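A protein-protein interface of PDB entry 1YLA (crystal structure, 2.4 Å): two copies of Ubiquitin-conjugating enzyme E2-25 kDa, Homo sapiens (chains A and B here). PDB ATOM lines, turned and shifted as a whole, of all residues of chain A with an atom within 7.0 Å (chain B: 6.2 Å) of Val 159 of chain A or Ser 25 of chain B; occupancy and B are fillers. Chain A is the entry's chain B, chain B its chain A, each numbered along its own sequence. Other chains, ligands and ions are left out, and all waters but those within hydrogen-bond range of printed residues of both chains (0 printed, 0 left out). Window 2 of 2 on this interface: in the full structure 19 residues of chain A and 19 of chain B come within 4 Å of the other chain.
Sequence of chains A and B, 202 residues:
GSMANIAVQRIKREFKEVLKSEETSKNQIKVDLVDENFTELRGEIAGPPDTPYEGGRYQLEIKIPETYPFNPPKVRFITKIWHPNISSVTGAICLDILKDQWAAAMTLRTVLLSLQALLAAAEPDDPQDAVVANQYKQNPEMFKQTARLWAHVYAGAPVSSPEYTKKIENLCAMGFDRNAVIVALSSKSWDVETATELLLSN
The side-chain amide nitrogen (ND2) of Asn 27 of chain B is in hydrogen-bond range of the backbone carbonyl oxygen (O) of Gly 156 of chain A (3.4 Å). The side-chain amide nitrogen (ND2) of Asn 27 of chain B is in hydrogen-bond range of the backbone carbonyl oxygen (O) of Ala 157 of chain A.
OG1 of Thr 24 of chain B sits at hydrogen-bond distance from O of Val 18 of chain B (2.7 Å). The side-chain hydroxyl of Ser 21 of chain B sits at hydrogen-bond distance from the side-chain hydroxyl of Thr 24 of chain B (2.9 Å). The backbone carbonyl oxygen (O) of Glu 22 of chain B is in hydrogen-bond range of the side-chain hydroxyl (OG) of Ser 25 of chain B. OG1 of Thr 24 of chain B sits at hydrogen-bond distance from O of Ile 29 of chain B (2.9 Å).
No position is printed for both chains.
Of the printed residues of chain B, His 152 of chain A touches Thr 24, Ser 25 and Asn 27. Printed residues of chain B within 4 Å of Ala 157 of chain A: Asn 27. Val 159 of chain A touches just these residues of chain B: Ser 25 and Asn 27. Glu 22 of chain B touches none of the printed residues of chain A. Of the printed residues of chain A, Thr 24 of chain B touches His 152 (3.5 Å). Of chain A, only His 152 and Val 159 come within 4 Å of Ser 25 of chain B. Of the printed residues of chain A, Asn 27 of chain B touches His 152, Gly 156, Ala 157, Pro 158 and Val 159. The nearest residue of chain A that does not touch Ser 25 of chain B is Pro 158 of chain A (5.4 Å). The nearest printed residue of chain A that does not touch Thr 24 of chain B is Val 159 of chain A (5.2 Å).
Hydrophobic or aromatic side chains of chain A that line the printed part of chain B: His 152 and Val 159. Of the 11 printed residues of chain B, 3 touch a printed residue of chain A. Among the printed residues, 8 pairs touch across the chains.
Among the printed residues, pairs that only touch across the chains: His 152 of chain A with Thr 24 of chain B (3.5 Å), His 152 of chain A with Ser 25 of chain B (3.8 Å), His 152 of chain A with Asn 27 of chain B (3.4 Å), Pro 158 of chain A with Asn 27 of chain B (3.7 Å), Val 159 of chain A with Ser 25 of chain B (3.0 Å) and Val 159 of chain A with Asn 27 of chain B (3.96 Å).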
ATOM      1  N   ARG A 148      15.256  -1.491  15.556  1.00  0.00           N
ATOM      2  CA  ARG A 148      16.503  -2.253  15.597  1.00  0.00           C
ATOM      3  C   ARG A 148      16.360  -3.609  14.908  1.00  0.00           C
ATOM      4  O   ARG A 148      17.341  -4.158  14.413  1.00  0.00           O
ATOM      5  CB  ARG A 148      16.976  -2.452  17.043  1.00  0.00           C
ATOM      6  CG  ARG A 148      17.907  -1.342  17.537  1.00  0.00           C
ATOM      7  CD  ARG A 148      18.257  -1.453  19.022  1.00  0.00           C
ATOM      8  NE  ARG A 148      18.884  -2.724  19.374  1.00  0.00           N
ATOM      9  CZ  ARG A 148      19.560  -2.941  20.503  1.00  0.00           C
ATOM     10  NH1 ARG A 148      19.702  -1.967  21.396  1.00  0.00           N
ATOM     11  NH2 ARG A 148      20.093  -4.136  20.748  1.00  0.00           N
ATOM     12  N   LEU A 149      15.147  -4.159  14.887  1.00  0.00           N
ATOM     13  CA  LEU A 149      14.907  -5.433  14.214  1.00  0.00           C
ATOM     14  C   LEU A 149      14.876  -5.175  12.711  1.00  0.00           C
ATOM     15  O   LEU A 149      15.447  -5.933  11.926  1.00  0.00           O
ATOM     16  CB  LEU A 149      13.570  -6.042  14.627  1.00  0.00           C
ATOM     17  CG  LEU A 149      13.313  -7.346  13.864  1.00  0.00           C
ATOM     18  CD1 LEU A 149      13.850  -8.533  14.664  1.00  0.00           C
ATOM     19  CD2 LEU A 149      11.835  -7.496  13.597  1.00  0.00           C
ATOM     20  N   HIS A 152      18.400  -4.794  11.411  1.00  0.00           N
ATOM     21  CA  HIS A 152      19.205  -5.994  11.242  1.00  0.00           C
ATOM     22  C   HIS A 152      18.729  -6.747  10.011  1.00  0.00           C
ATOM     23  O   HIS A 152      19.537  -7.254   9.230  1.00  0.00           O
ATOM     24  CB  HIS A 152      19.124  -6.922  12.464  1.00  0.00           C
ATOM     25  CG  HIS A 152      19.633  -8.307  12.193  1.00  0.00           C
ATOM     26  ND1 HIS A 152      18.796  -9.393  12.044  1.00  0.00           N
ATOM     27  CD2 HIS A 152      20.885  -8.766  11.951  1.00  0.00           C
ATOM     28  CE1 HIS A 152      19.508 -10.459  11.717  1.00  0.00           C
ATOM     29  NE2 HIS A 152      20.779 -10.105  11.654  1.00  0.00           N
ATOM     30  N   VAL A 153      17.414  -6.807   9.830  1.00  0.00           N
ATOM     31  CA  VAL A 153      16.837  -7.524   8.696  1.00  0.00           C
ATOM     32  C   VAL A 153      17.018  -6.886   7.320  1.00  0.00           C
ATOM     33  O   VAL A 153      17.295  -7.591   6.359  1.00  0.00           O
ATOM     34  CB  VAL A 153      15.328  -7.804   8.933  1.00  0.00           C
ATOM     35  CG1 VAL A 153      14.681  -8.320   7.662  1.00  0.00           C
ATOM     36  CG2 VAL A 153      15.169  -8.826  10.060  1.00  0.00           C
ATOM     37  N   GLY A 156      21.336  -4.495   7.735  1.00  0.00           N
ATOM     38  CA  GLY A 156      22.553  -5.174   8.133  1.00  0.00           C
ATOM     39  C   GLY A 156      23.157  -4.791   9.471  1.00  0.00           C
ATOM     40  O   GLY A 156      24.363  -4.959   9.669  1.00  0.00           O
ATOM     41  N   ALA A 157      22.342  -4.267  10.384  1.00  0.00           N
ATOM     42  CA  ALA A 157      22.821  -3.907  11.717  1.00  0.00           C
ATOM     43  C   ALA A 157      22.900  -5.217  12.500  1.00  0.00           C
ATOM     44  O   ALA A 157      22.281  -6.209  12.121  1.00  0.00           O
ATOM     45  CB  ALA A 157      21.846  -2.947  12.389  1.00  0.00           C
ATOM     46  N   PRO A 158      23.671  -5.251  13.592  1.00  0.00           N
ATOM     47  CA  PRO A 158      23.767  -6.500  14.368  1.00  0.00           C
ATOM     48  C   PRO A 158      22.385  -7.087  14.708  1.00  0.00           C
ATOM     49  O   PRO A 158      21.374  -6.378  14.672  1.00  0.00           O
ATOM     50  CB  PRO A 158      24.544  -6.068  15.606  1.00  0.00           C
ATOM     51  CG  PRO A 158      25.435  -4.976  15.069  1.00  0.00           C
ATOM     52  CD  PRO A 158      24.504  -4.189  14.180  1.00  0.00           C
ATOM     53  N   VAL A 159      22.334  -8.381  15.028  1.00  0.00           N
ATOM     54  CA  VAL A 159      21.055  -9.023  15.351  1.00  0.00           C
ATOM     55  C   VAL A 159      20.300  -8.307  16.472  1.00  0.00           C
ATOM     56  O   VAL A 159      20.852  -7.424  17.136  1.00  0.00           O
ATOM     57  CB  VAL A 159      21.238 -10.504  15.756  1.00  0.00           C
ATOM     58  CG1 VAL A 159      20.689 -11.408  14.667  1.00  0.00           C
ATOM     59  CG2 VAL A 159      22.707 -10.801  16.006  1.00  0.00           C
ATOM     60  N   SER A 160      19.040  -8.692  16.680  1.00  0.00           N
ATOM     61  CA  SER A 160      18.221  -8.070  17.716  1.00  0.00           C
ATOM     62  C   SER A 160      16.816  -8.671  17.881  1.00  0.00           C
ATOM     63  O   SER A 160      16.037  -8.725  16.924  1.00  0.00           O
ATOM     64  CB  SER A 160      18.097  -6.562  17.430  1.00  0.00           C
ATOM     65  OG  SER A 160      17.717  -5.833  18.588  1.00  0.00           O
ATOM     66  N   SER A 161      16.515  -9.124  19.099  1.00  0.00           N
ATOM     67  CA  SER A 161      15.203  -9.671  19.463  1.00  0.00           C
ATOM     68  C   SER A 161      14.825 -11.093  19.091  1.00  0.00           C
ATOM     69  O   SER A 161      14.142 -11.320  18.095  1.00  0.00           O
ATOM     70  CB  SER A 161      14.092  -8.746  18.960  1.00  0.00           C
ATOM     71  OG  SER A 161      14.123  -7.504  19.642  1.00  0.00           O
ATOM     72  N   THR A 165      11.955 -12.402  16.190  1.00  0.00           N
ATOM     73  CA  THR A 165      12.327 -13.281  15.102  1.00  0.00           C
ATOM     74  C   THR A 165      11.533 -14.585  15.138  1.00  0.00           C
ATOM     75  O   THR A 165      11.184 -15.117  14.088  1.00  0.00           O
ATOM     76  CB  THR A 165      13.839 -13.581  15.141  1.00  0.00           C
ATOM     77  OG1 THR A 165      14.140 -14.350  16.310  1.00  0.00           O
ATOM     78  CG2 THR A 165      14.636 -12.281  15.195  1.00  0.00           C
ATOM     79  N   VAL B  18      18.149 -20.242   4.912  1.00  0.00           N
ATOM     80  CA  VAL B  18      19.112 -19.143   4.951  1.00  0.00           C
ATOM     81  C   VAL B  18      18.703 -18.141   6.010  1.00  0.00           C
ATOM     82  O   VAL B  18      19.538 -17.652   6.768  1.00  0.00           O
ATOM     83  CB  VAL B  18      19.219 -18.399   3.580  1.00  0.00           C
ATOM     84  CG1 VAL B  18      19.719 -16.968   3.785  1.00  0.00           C
ATOM     85  CG2 VAL B  18      20.186 -19.141   2.657  1.00  0.00           C
ATOM     86  N   LEU B  19      17.408 -17.848   6.053  1.00  0.00           N
ATOM     87  CA  LEU B  19      16.863 -16.893   7.002  1.00  0.00           C
ATOM     88  C   LEU B  19      17.019 -17.342   8.446  1.00  0.00           C
ATOM     89  O   LEU B  19      16.984 -16.513   9.354  1.00  0.00           O
ATOM     90  CB  LEU B  19      15.381 -16.642   6.702  1.00  0.00           C
ATOM     91  CG  LEU B  19      15.014 -16.119   5.308  1.00  0.00           C
ATOM     92  CD1 LEU B  19      13.523 -15.837   5.255  1.00  0.00           C
ATOM     93  CD2 LEU B  19      15.780 -14.860   4.998  1.00  0.00           C
ATOM     94  N   SER B  21      19.719 -19.347   9.499  1.00  0.00           N
ATOM     95  CA  SER B  21      21.091 -19.799   9.702  1.00  0.00           C
ATOM     96  C   SER B  21      21.840 -18.989  10.766  1.00  0.00           C
ATOM     97  O   SER B  21      21.490 -17.843  11.043  1.00  0.00           O
ATOM     98  CB  SER B  21      21.847 -19.710   8.377  1.00  0.00           C
ATOM     99  OG  SER B  21      21.737 -18.409   7.826  1.00  0.00           O
ATOM    100  N   GLU B  22      22.858 -19.591  11.372  1.00  0.00           N
ATOM    101  CA  GLU B  22      23.661 -18.877  12.350  1.00  0.00           C
ATOM    102  C   GLU B  22      24.482 -17.812  11.601  1.00  0.00           C
ATOM    103  O   GLU B  22      24.849 -16.781  12.164  1.00  0.00           O
ATOM    104  CB  GLU B  22      24.613 -19.831  13.076  1.00  0.00           C
ATOM    105  CG  GLU B  22      23.947 -20.739  14.098  1.00  0.00           C
ATOM    106  CD  GLU B  22      24.960 -21.453  14.994  1.00  0.00           C
ATOM    107  OE1 GLU B  22      24.539 -22.239  15.866  1.00  0.00           O
ATOM    108  OE2 GLU B  22      26.178 -21.226  14.827  1.00  0.00           O
ATOM    109  N   GLU B  23      24.759 -18.069  10.323  1.00  0.00           N
ATOM    110  CA  GLU B  23      25.543 -17.153   9.496  1.00  0.00           C
ATOM    111  C   GLU B  23      24.787 -15.869   9.186  1.00  0.00           C
ATOM    112  O   GLU B  23      25.385 -14.799   9.092  1.00  0.00           O
ATOM    113  CB  GLU B  23      25.964 -17.835   8.190  1.00  0.00           C
ATOM    114  CG  GLU B  23      26.892 -19.032   8.386  1.00  0.00           C
ATOM    115  CD  GLU B  23      26.170 -20.377   8.413  1.00  0.00           C
ATOM    116  OE1 GLU B  23      26.856 -21.415   8.513  1.00  0.00           O
ATOM    117  OE2 GLU B  23      24.927 -20.404   8.325  1.00  0.00           O
ATOM    118  N   THR B  24      23.474 -15.977   9.020  1.00  0.00           N
ATOM    119  CA  THR B  24      22.657 -14.807   8.746  1.00  0.00           C
ATOM    120  C   THR B  24      22.469 -13.997  10.016  1.00  0.00           C
ATOM    121  O   THR B  24      22.412 -12.766   9.966  1.00  0.00           O
ATOM    122  CB  THR B  24      21.273 -15.196   8.203  1.00  0.00           C
ATOM    123  OG1 THR B  24      21.412 -15.678   6.865  1.00  0.00           O
ATOM    124  CG2 THR B  24      20.341 -14.001   8.181  1.00  0.00           C
ATOM    125  N   SER B  25      22.377 -14.686  11.154  1.00  0.00           N
ATOM    126  CA  SER B  25      22.181 -14.012  12.431  1.00  0.00           C
ATOM    127  C   SER B  25      23.422 -13.215  12.773  1.00  0.00           C
ATOM    128  O   SER B  25      23.358 -12.234  13.510  1.00  0.00           O
ATOM    129  CB  SER B  25      21.885 -15.021  13.541  1.00  0.00           C
ATOM    130  OG  SER B  25      23.023 -15.799  13.846  1.00  0.00           O
ATOM    131  N   LYS B  26      24.550 -13.646  12.221  1.00  0.00           N
ATOM    132  CA  LYS B  26      25.835 -12.988  12.429  1.00  0.00           C
ATOM    133  C   LYS B  26      26.150 -12.106  11.217  1.00  0.00           C
ATOM    134  O   LYS B  26      27.302 -11.766  10.965  1.00  0.00           O
ATOM    135  CB  LYS B  26      26.933 -14.048  12.612  1.00  0.00           C
ATOM    136  CG  LYS B  26      26.721 -14.939  13.824  1.00  0.00           C
ATOM    137  CD  LYS B  26      27.677 -16.111  13.853  1.00  0.00           C
ATOM    138  CE  LYS B  26      27.374 -17.017  15.054  1.00  0.00           C
ATOM    139  NZ  LYS B  26      28.233 -18.241  15.153  1.00  0.00           N
ATOM    140  N   ASN B  27      25.117 -11.745  10.468  1.00  0.00           N
ATOM    141  CA  ASN B  27      25.259 -10.925   9.267  1.00  0.00           C
ATOM    142  C   ASN B  27      26.347 -11.352   8.284  1.00  0.00           C
ATOM    143  O   ASN B  27      27.051 -10.504   7.755  1.00  0.00           O
ATOM    144  CB  ASN B  27      25.492  -9.464   9.644  1.00  0.00           C
ATOM    145  CG  ASN B  27      24.361  -8.892  10.453  1.00  0.00           C
ATOM    146  OD1 ASN B  27      24.332  -9.024  11.671  1.00  0.00           O
ATOM    147  ND2 ASN B  27      23.404  -8.269   9.777  1.00  0.00           N
ATOM    148  N   GLN B  28      26.494 -12.649   8.027  1.00  0.00           N
ATOM    149  CA  GLN B  28      27.510 -13.101   7.079  1.00  0.00           C
ATOM    150  C   GLN B  28      26.877 -13.314   5.710  1.00  0.00           C
ATOM    151  O   GLN B  28      27.509 -13.098   4.680  1.00  0.00           O
ATOM    152  CB  GLN B  28      28.183 -14.400   7.552  1.00  0.00           C
ATOM    153  CG  GLN B  28      29.100 -14.252   8.763  1.00  0.00           C
ATOM    154  CD  GLN B  28      30.102 -13.107   8.624  1.00  0.00           C
ATOM    155  OE1 GLN B  28      30.977 -13.116   7.743  1.00  0.00           O
ATOM    156  NE2 GLN B  28      29.977 -12.109   9.499  1.00  0.00           N
ATOM    157  N   ILE B  29      25.623 -13.748   5.703  1.00  0.00           N
ATOM    158  CA  ILE B  29      24.914 -13.969   4.450  1.00  0.00           C
ATOM    159  C   ILE B  29      23.450 -13.586   4.616  1.00  0.00           C
ATOM    160  O   ILE B  29      22.946 -13.486   5.729  1.00  0.00           O
ATOM    161  CB  ILE B  29      25.004 -15.461   3.966  1.00  0.00           C
ATOM    162  CG1 ILE B  29      24.127 -16.375   4.834  1.00  0.00           C
ATOM    163  CG2 ILE B  29      26.450 -15.933   3.996  1.00  0.00           C
ATOM    164  CD1 ILE B  29      24.042 -17.828   4.330  1.00  0.00           C
